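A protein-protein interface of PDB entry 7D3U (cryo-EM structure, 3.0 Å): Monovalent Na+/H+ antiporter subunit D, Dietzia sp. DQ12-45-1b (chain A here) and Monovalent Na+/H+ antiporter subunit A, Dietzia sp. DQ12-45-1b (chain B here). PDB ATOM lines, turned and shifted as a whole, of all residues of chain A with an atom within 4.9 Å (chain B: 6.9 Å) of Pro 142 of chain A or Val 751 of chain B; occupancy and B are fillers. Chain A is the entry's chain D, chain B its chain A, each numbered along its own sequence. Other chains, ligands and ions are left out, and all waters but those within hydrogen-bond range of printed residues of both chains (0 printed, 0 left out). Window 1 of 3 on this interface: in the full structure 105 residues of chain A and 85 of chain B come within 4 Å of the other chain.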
ATOM      1  N   LEU A 112      11.962 -17.415 -21.090  1.00  0.00           N
ATOM      2  CA  LEU A 112      12.437 -17.429 -22.470  1.00  0.00           C
ATOM      3  C   LEU A 112      12.738 -18.846 -22.940  1.00  0.00           C
ATOM      4  O   LEU A 112      12.491 -19.181 -24.103  1.00  0.00           O
ATOM      5  CB  LEU A 112      13.667 -16.537 -22.612  1.00  0.00           C
ATOM      6  CG  LEU A 112      13.389 -15.035 -22.636  1.00  0.00           C
ATOM      7  CD1 LEU A 112      14.677 -14.259 -22.827  1.00  0.00           C
ATOM      8  CD2 LEU A 112      12.387 -14.689 -23.718  1.00  0.00           C
ATOM      9  N   LEU A 115       9.429 -20.330 -23.788  1.00  0.00           N
ATOM     10  CA  LEU A 115       8.901 -19.793 -25.036  1.00  0.00           C
ATOM     11  C   LEU A 115       9.631 -20.375 -26.240  1.00  0.00           C
ATOM     12  O   LEU A 115       9.008 -20.672 -27.267  1.00  0.00           O
ATOM     13  CB  LEU A 115       8.993 -18.269 -25.023  1.00  0.00           C
ATOM     14  CG  LEU A 115       7.931 -17.582 -24.165  1.00  0.00           C
ATOM     15  CD1 LEU A 115       8.510 -16.398 -23.418  1.00  0.00           C
ATOM     16  CD2 LEU A 115       6.768 -17.141 -25.026  1.00  0.00           C
ATOM     17  N   VAL A 116      10.947 -20.565 -26.128  1.00  0.00           N
ATOM     18  CA  VAL A 116      11.697 -21.233 -27.189  1.00  0.00           C
ATOM     19  C   VAL A 116      11.217 -22.668 -27.357  1.00  0.00           C
ATOM     20  O   VAL A 116      11.076 -23.165 -28.480  1.00  0.00           O
ATOM     21  CB  VAL A 116      13.206 -21.167 -26.896  1.00  0.00           C
ATOM     22  CG1 VAL A 116      13.982 -21.957 -27.919  1.00  0.00           C
ATOM     23  CG2 VAL A 116      13.679 -19.733 -26.898  1.00  0.00           C
ATOM     24  N   GLU A 137       9.473 -17.893 -35.945  1.00  0.00           N
ATOM     25  CA  GLU A 137       9.695 -16.603 -35.290  1.00  0.00           C
ATOM     26  C   GLU A 137       9.447 -16.691 -33.788  1.00  0.00           C
ATOM     27  O   GLU A 137      10.137 -16.032 -33.001  1.00  0.00           O
ATOM     28  CB  GLU A 137       8.827 -15.521 -35.925  1.00  0.00           C
ATOM     29  CG  GLU A 137       8.762 -15.616 -37.431  1.00  0.00           C
ATOM     30  CD  GLU A 137      10.132 -15.629 -38.079  1.00  0.00           C
ATOM     31  OE1 GLU A 137      11.077 -15.032 -37.518  1.00  0.00           O
ATOM     32  OE2 GLU A 137      10.274 -16.278 -39.133  1.00  0.00           O
ATOM     33  N   VAL A 138       8.462 -17.488 -33.369  1.00  0.00           N
ATOM     34  CA  VAL A 138       8.224 -17.716 -31.946  1.00  0.00           C
ATOM     35  C   VAL A 138       9.411 -18.414 -31.299  1.00  0.00           C
ATOM     36  O   VAL A 138       9.637 -18.272 -30.095  1.00  0.00           O
ATOM     37  CB  VAL A 138       6.925 -18.526 -31.742  1.00  0.00           C
ATOM     38  CG1 VAL A 138       6.688 -18.823 -30.270  1.00  0.00           C
ATOM     39  CG2 VAL A 138       5.752 -17.774 -32.305  1.00  0.00           C
ATOM     40  N   MET A 139      10.169 -19.182 -32.073  1.00  0.00           N
ATOM     41  CA  MET A 139      11.389 -19.807 -31.583  1.00  0.00           C
ATOM     42  C   MET A 139      12.584 -18.866 -31.625  1.00  0.00           C
ATOM     43  O   MET A 139      13.484 -18.977 -30.785  1.00  0.00           O
ATOM     44  CB  MET A 139      11.693 -21.061 -32.407  1.00  0.00           C
ATOM     45  CG  MET A 139      12.948 -21.802 -32.001  1.00  0.00           C
ATOM     46  SD  MET A 139      13.460 -22.980 -33.262  1.00  0.00           S
ATOM     47  CE  MET A 139      13.821 -21.879 -34.624  1.00  0.00           C
ATOM     48  N   LEU A 140      12.605 -17.934 -32.578  1.00  0.00           N
ATOM     49  CA  LEU A 140      13.769 -17.075 -32.761  1.00  0.00           C
ATOM     50  C   LEU A 140      13.749 -15.872 -31.829  1.00  0.00           C
ATOM     51  O   LEU A 140      14.803 -15.442 -31.352  1.00  0.00           O
ATOM     52  CB  LEU A 140      13.852 -16.606 -34.212  1.00  0.00           C
ATOM     53  CG  LEU A 140      14.435 -17.591 -35.222  1.00  0.00           C
ATOM     54  CD1 LEU A 140      14.442 -16.975 -36.608  1.00  0.00           C
ATOM     55  CD2 LEU A 140      15.833 -18.001 -34.811  1.00  0.00           C
ATOM     56  N   LEU A 141      12.573 -15.302 -31.571  1.00  0.00           N
ATOM     57  CA  LEU A 141      12.519 -14.104 -30.737  1.00  0.00           C
ATOM     58  C   LEU A 141      13.011 -14.340 -29.313  1.00  0.00           C
ATOM     59  O   LEU A 141      13.807 -13.518 -28.825  1.00  0.00           O
ATOM     60  CB  LEU A 141      11.099 -13.526 -30.744  1.00  0.00           C
ATOM     61  CG  LEU A 141      10.792 -12.597 -31.915  1.00  0.00           C
ATOM     62  CD1 LEU A 141      10.811 -13.364 -33.225  1.00  0.00           C
ATOM     63  CD2 LEU A 141       9.451 -11.930 -31.704  1.00  0.00           C
ATOM     64  N   PRO A 142      12.600 -15.393 -28.595  1.00  0.00           N
ATOM     65  CA  PRO A 142      13.219 -15.658 -27.289  1.00  0.00           C
ATOM     66  C   PRO A 142      14.668 -16.063 -27.396  1.00  0.00           C
ATOM     67  O   PRO A 142      15.401 -15.943 -26.409  1.00  0.00           O
ATOM     68  CB  PRO A 142      12.365 -16.794 -26.715  1.00  0.00           C
ATOM     69  CG  PRO A 142      11.099 -16.742 -27.471  1.00  0.00           C
ATOM     70  CD  PRO A 142      11.476 -16.305 -28.841  1.00  0.00           C
ATOM     71  N   SER A 143      15.104 -16.547 -28.556  1.00  0.00           N
ATOM     72  CA  SER A 143      16.519 -16.839 -28.735  1.00  0.00           C
ATOM     73  C   SER A 143      17.346 -15.564 -28.697  1.00  0.00           C
ATOM     74  O   SER A 143      18.462 -15.558 -28.168  1.00  0.00           O
ATOM     75  CB  SER A 143      16.741 -17.581 -30.046  1.00  0.00           C
ATOM     76  OG  SER A 143      15.733 -18.550 -30.260  1.00  0.00           O
ATOM     77  N   TYR A 144      16.814 -14.473 -29.249  1.00  0.00           N
ATOM     78  CA  TYR A 144      17.542 -13.211 -29.229  1.00  0.00           C
ATOM     79  C   TYR A 144      17.662 -12.664 -27.815  1.00  0.00           C
ATOM     80  O   TYR A 144      18.675 -12.042 -27.476  1.00  0.00           O
ATOM     81  CB  TYR A 144      16.858 -12.191 -30.137  1.00  0.00           C
ATOM     82  CG  TYR A 144      16.621 -12.678 -31.549  1.00  0.00           C
ATOM     83  CD1 TYR A 144      17.427 -13.655 -32.115  1.00  0.00           C
ATOM     84  CD2 TYR A 144      15.590 -12.156 -32.316  1.00  0.00           C
ATOM     85  CE1 TYR A 144      17.212 -14.100 -33.402  1.00  0.00           C
ATOM     86  CE2 TYR A 144      15.368 -12.595 -33.604  1.00  0.00           C
ATOM     87  CZ  TYR A 144      16.181 -13.566 -34.142  1.00  0.00           C
ATOM     88  OH  TYR A 144      15.964 -14.007 -35.426  1.00  0.00           O
ATOM     89  N   GLY A 145      16.645 -12.880 -26.980  1.00  0.00           N
ATOM     90  CA  GLY A 145      16.748 -12.478 -25.591  1.00  0.00           C
ATOM     91  C   GLY A 145      17.730 -13.321 -24.807  1.00  0.00           C
ATOM     92  O   GLY A 145      18.407 -12.815 -23.908  1.00  0.00           O
ATOM     93  N   LEU A 146      17.829 -14.611 -25.134  1.00  0.00           N
ATOM     94  CA  LEU A 146      18.773 -15.486 -24.451  1.00  0.00           C
ATOM     95  C   LEU A 146      20.215 -15.191 -24.831  1.00  0.00           C
ATOM     96  O   LEU A 146      21.126 -15.558 -24.082  1.00  0.00           O
ATOM     97  CB  LEU A 146      18.450 -16.948 -24.754  1.00  0.00           C
ATOM     98  CG  LEU A 146      17.197 -17.521 -24.096  1.00  0.00           C
ATOM     99  CD1 LEU A 146      17.011 -18.973 -24.489  1.00  0.00           C
ATOM    100  CD2 LEU A 146      17.287 -17.381 -22.594  1.00  0.00           C
ATOM    101  N   LEU B 746       1.576 -12.756 -30.883  1.00  0.00           N
ATOM    102  CA  LEU B 746       1.451 -11.951 -29.673  1.00  0.00           C
ATOM    103  C   LEU B 746       2.543 -12.380 -28.700  1.00  0.00           C
ATOM    104  O   LEU B 746       3.115 -11.543 -27.989  1.00  0.00           O
ATOM    105  CB  LEU B 746       0.059 -12.100 -29.051  1.00  0.00           C
ATOM    106  CG  LEU B 746      -0.508 -13.446 -28.591  1.00  0.00           C
ATOM    107  CD1 LEU B 746       0.037 -13.846 -27.230  1.00  0.00           C
ATOM    108  CD2 LEU B 746      -2.022 -13.391 -28.549  1.00  0.00           C
ATOM    109  N   THR B 747       2.868 -13.676 -28.674  1.00  0.00           N
ATOM    110  CA  THR B 747       3.993 -14.118 -27.860  1.00  0.00           C
ATOM    111  C   THR B 747       5.302 -13.560 -28.397  1.00  0.00           C
ATOM    112  O   THR B 747       6.196 -13.211 -27.623  1.00  0.00           O
ATOM    113  CB  THR B 747       4.043 -15.643 -27.800  1.00  0.00           C
ATOM    114  OG1 THR B 747       3.654 -16.183 -29.066  1.00  0.00           O
ATOM    115  CG2 THR B 747       3.098 -16.153 -26.731  1.00  0.00           C
ATOM    116  N   VAL B 748       5.428 -13.457 -29.722  1.00  0.00           N
ATOM    117  CA  VAL B 748       6.613 -12.848 -30.321  1.00  0.00           C
ATOM    118  C   VAL B 748       6.764 -11.406 -29.861  1.00  0.00           C
ATOM    119  O   VAL B 748       7.861 -10.966 -29.502  1.00  0.00           O
ATOM    120  CB  VAL B 748       6.545 -12.943 -31.856  1.00  0.00           C
ATOM    121  CG1 VAL B 748       6.574 -14.391 -32.300  1.00  0.00           C
ATOM    122  CG2 VAL B 748       5.294 -12.271 -32.367  1.00  0.00           C
ATOM    123  N   LEU B 749       5.669 -10.648 -29.864  1.00  0.00           N
ATOM    124  CA  LEU B 749       5.743  -9.252 -29.441  1.00  0.00           C
ATOM    125  C   LEU B 749       6.096  -9.141 -27.961  1.00  0.00           C
ATOM    126  O   LEU B 749       6.969  -8.350 -27.579  1.00  0.00           O
ATOM    127  CB  LEU B 749       4.426  -8.539 -29.742  1.00  0.00           C
ATOM    128  CG  LEU B 749       4.546  -7.460 -30.817  1.00  0.00           C
ATOM    129  CD1 LEU B 749       3.304  -6.602 -30.868  1.00  0.00           C
ATOM    130  CD2 LEU B 749       5.767  -6.600 -30.567  1.00  0.00           C
ATOM    131  N   GLY B 750       5.419  -9.917 -27.111  1.00  0.00           N
ATOM    132  CA  GLY B 750       5.765  -9.915 -25.698  1.00  0.00           C
ATOM    133  C   GLY B 750       7.217 -10.280 -25.455  1.00  0.00           C
ATOM    134  O   GLY B 750       7.891  -9.688 -24.605  1.00  0.00           O
ATOM    135  N   VAL B 751       7.725 -11.250 -26.213  1.00  0.00           N
ATOM    136  CA  VAL B 751       9.114 -11.656 -26.073  1.00  0.00           C
ATOM    137  C   VAL B 751      10.044 -10.544 -26.531  1.00  0.00           C
ATOM    138  O   VAL B 751      11.105 -10.331 -25.943  1.00  0.00           O
ATOM    139  CB  VAL B 751       9.360 -12.957 -26.852  1.00  0.00           C
ATOM    140  CG1 VAL B 751      10.824 -13.140 -27.084  1.00  0.00           C
ATOM    141  CG2 VAL B 751       8.800 -14.132 -26.088  1.00  0.00           C
ATOM    142  N   ALA B 752       9.670  -9.822 -27.586  1.00  0.00           N
ATOM    143  CA  ALA B 752      10.487  -8.694 -28.021  1.00  0.00           C
ATOM    144  C   ALA B 752      10.541  -7.621 -26.945  1.00  0.00           C
ATOM    145  O   ALA B 752      11.583  -6.990 -26.738  1.00  0.00           O
ATOM    146  CB  ALA B 752       9.947  -8.119 -29.328  1.00  0.00           C
ATOM    147  N   GLY B 753       9.431  -7.410 -26.240  1.00  0.00           N
ATOM    148  CA  GLY B 753       9.450  -6.478 -25.121  1.00  0.00           C
ATOM    149  C   GLY B 753      10.380  -6.929 -24.009  1.00  0.00           C
ATOM    150  O   GLY B 753      11.209  -6.156 -23.512  1.00  0.00           O
ATOM    151  N   LEU B 754      10.254  -8.196 -23.605  1.00  0.00           N
ATOM    152  CA  LEU B 754      11.140  -8.733 -22.575  1.00  0.00           C
ATOM    153  C   LEU B 754      12.599  -8.668 -23.013  1.00  0.00           C
ATOM    154  O   LEU B 754      13.493  -8.421 -22.196  1.00  0.00           O
ATOM    155  CB  LEU B 754      10.754 -10.172 -22.240  1.00  0.00           C
ATOM    156  CG  LEU B 754       9.324 -10.412 -21.764  1.00  0.00           C
ATOM    157  CD1 LEU B 754       9.151 -11.855 -21.333  1.00  0.00           C
ATOM    158  CD2 LEU B 754       8.976  -9.466 -20.630  1.00  0.00           C
ATOM    159  N   ALA B 755      12.857  -8.875 -24.302  1.00  0.00           N
ATOM    160  CA  ALA B 755      14.222  -8.863 -24.803  1.00  0.00           C
ATOM    161  C   ALA B 755      14.781  -7.452 -24.865  1.00  0.00           C
ATOM    162  O   ALA B 755      15.975  -7.256 -24.637  1.00  0.00           O
ATOM    163  CB  ALA B 755      14.279  -9.526 -26.177  1.00  0.00           C
ATOM    164  N   VAL B 756      13.943  -6.460 -25.169  1.00  0.00           N
ATOM    165  CA  VAL B 756      14.370  -5.070 -25.057  1.00  0.00           C
ATOM    166  C   VAL B 756      14.744  -4.753 -23.616  1.00  0.00           C
ATOM    167  O   VAL B 756      15.765  -4.103 -23.348  1.00  0.00           O
ATOM    168  CB  VAL B 756      13.268  -4.128 -25.576  1.00  0.00           C
ATOM    169  CG1 VAL B 756      13.479  -2.717 -25.058  1.00  0.00           C
ATOM    170  CG2 VAL B 756      13.231  -4.142 -27.089  1.00  0.00           C
ATOM    171  N   ILE B 757      13.925  -5.213 -22.667  1.00  0.00           N
ATOM    172  CA  ILE B 757      14.237  -5.007 -21.253  1.00  0.00           C
ATOM    173  C   ILE B 757      15.587  -5.627 -20.910  1.00  0.00           C
ATOM    174  O   ILE B 757      16.446  -4.991 -20.287  1.00  0.00           O
ATOM    175  CB  ILE B 757      13.117  -5.576 -20.365  1.00  0.00           C
ATOM    176  CG1 ILE B 757      11.821  -4.798 -20.576  1.00  0.00           C
ATOM    177  CG2 ILE B 757      13.526  -5.533 -18.907  1.00  0.00           C
ATOM    178  CD1 ILE B 757      10.748  -5.134 -19.572  1.00  0.00           C
ATOM    179  N   ILE B 854       2.651  -7.491 -19.907  1.00  0.00           N
ATOM    180  CA  ILE B 854       2.962  -8.490 -20.927  1.00  0.00           C
ATOM    181  C   ILE B 854       2.621  -9.884 -20.425  1.00  0.00           C
ATOM    182  O   ILE B 854       2.034 -10.701 -21.151  1.00  0.00           O
ATOM    183  CB  ILE B 854       4.443  -8.392 -21.338  1.00  0.00           C
ATOM    184  CG1 ILE B 854       4.731  -7.053 -22.012  1.00  0.00           C
ATOM    185  CG2 ILE B 854       4.815  -9.539 -22.255  1.00  0.00           C
ATOM    186  CD1 ILE B 854       6.202  -6.761 -22.159  1.00  0.00           C
ATOM    187  N   VAL B 858      -0.177 -12.368 -22.204  1.00  0.00           N
ATOM    188  CA  VAL B 858       0.118 -13.711 -22.695  1.00  0.00           C
ATOM    189  C   VAL B 858      -0.693 -14.751 -21.929  1.00  0.00           C
ATOM    190  O   VAL B 858      -1.194 -15.718 -22.514  1.00  0.00           O
ATOM    191  CB  VAL B 858       1.628 -13.993 -22.614  1.00  0.00           C
ATOM    192  CG1 VAL B 858       1.924 -15.421 -23.038  1.00  0.00           C
ATOM    193  CG2 VAL B 858       2.394 -13.013 -23.483  1.00  0.00           C
ATOM    194  N   VAL B 904       4.251  -4.136 -24.494  1.00  0.00           N
ATOM    195  CA  VAL B 904       5.456  -4.074 -25.318  1.00  0.00           C
ATOM    196  C   VAL B 904       5.779  -2.632 -25.686  1.00  0.00           C
ATOM    197  O   VAL B 904       6.937  -2.199 -25.608  1.00  0.00           O
ATOM    198  CB  VAL B 904       5.297  -4.949 -26.571  1.00  0.00           C
ATOM    199  CG1 VAL B 904       6.514  -4.803 -27.468  1.00  0.00           C
ATOM    200  CG2 VAL B 904       5.100  -6.385 -26.167  1.00  0.00           C
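Among the printed residues, merely in contact across the chains: Leu 141 of chain A with Val 748 of chain B (2.9 Å), Pro 142 of chain A with Val 751 of chain B (3.2 Å), Leu 141 of chain A with Val 751 of chain B (3.3 Å), Val 138 of chain A with Val 748 of chain B (3.5 Å), Leu 115 of chain A with Val 751 of chain B (3.5 Å), Gly 145 of chain A with Ala 755 of chain B (3.9 Å) and Glu 137 of chain A with Val 748 of chain B (3.97 Å).
Of chain B, only Val 751 (3.2 Å) comes within 4 Å of Pro 142 of chain A. Val 751 of chain B touches just these residues of chain A: Leu 115 (3.5 Å), Leu 141 (3.3 Å) and Pro 142 (3.2 Å). Printed residues of chain A within 4 Å of Ala 755 of chain B: Gly 145. Of the printed residues of chain B, Leu 115 of chain A touches Val 751. Printed residues of chain B within 4 Å of Val 138 of chain A: Val 748. Of the printed residues of chain B, Glu 137 of chain A touches Val 748. Of the printed residues of chain B, Leu 141 of chain A touches Val 748 and Val 751. Ile 854 of chain B touches none of the printed residues of chain A. Gly 753 of chain B touches none of the printed residues of chain A. The nearest residue of chain B that does not touch Pro 142 of chain A is Thr 747 of chain B (6.0 Å). The nearest printed residue of chain B that does not touch Val 138 of chain A is Thr 747 of chain B (4.2 Å).
Hydrophobic or aromatic side chains of chain B that line the printed part of chain A: Val 748, Val 751 and Ala 755. Of the 13 printed residues of chain A, 6 touch a printed residue of chain B.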
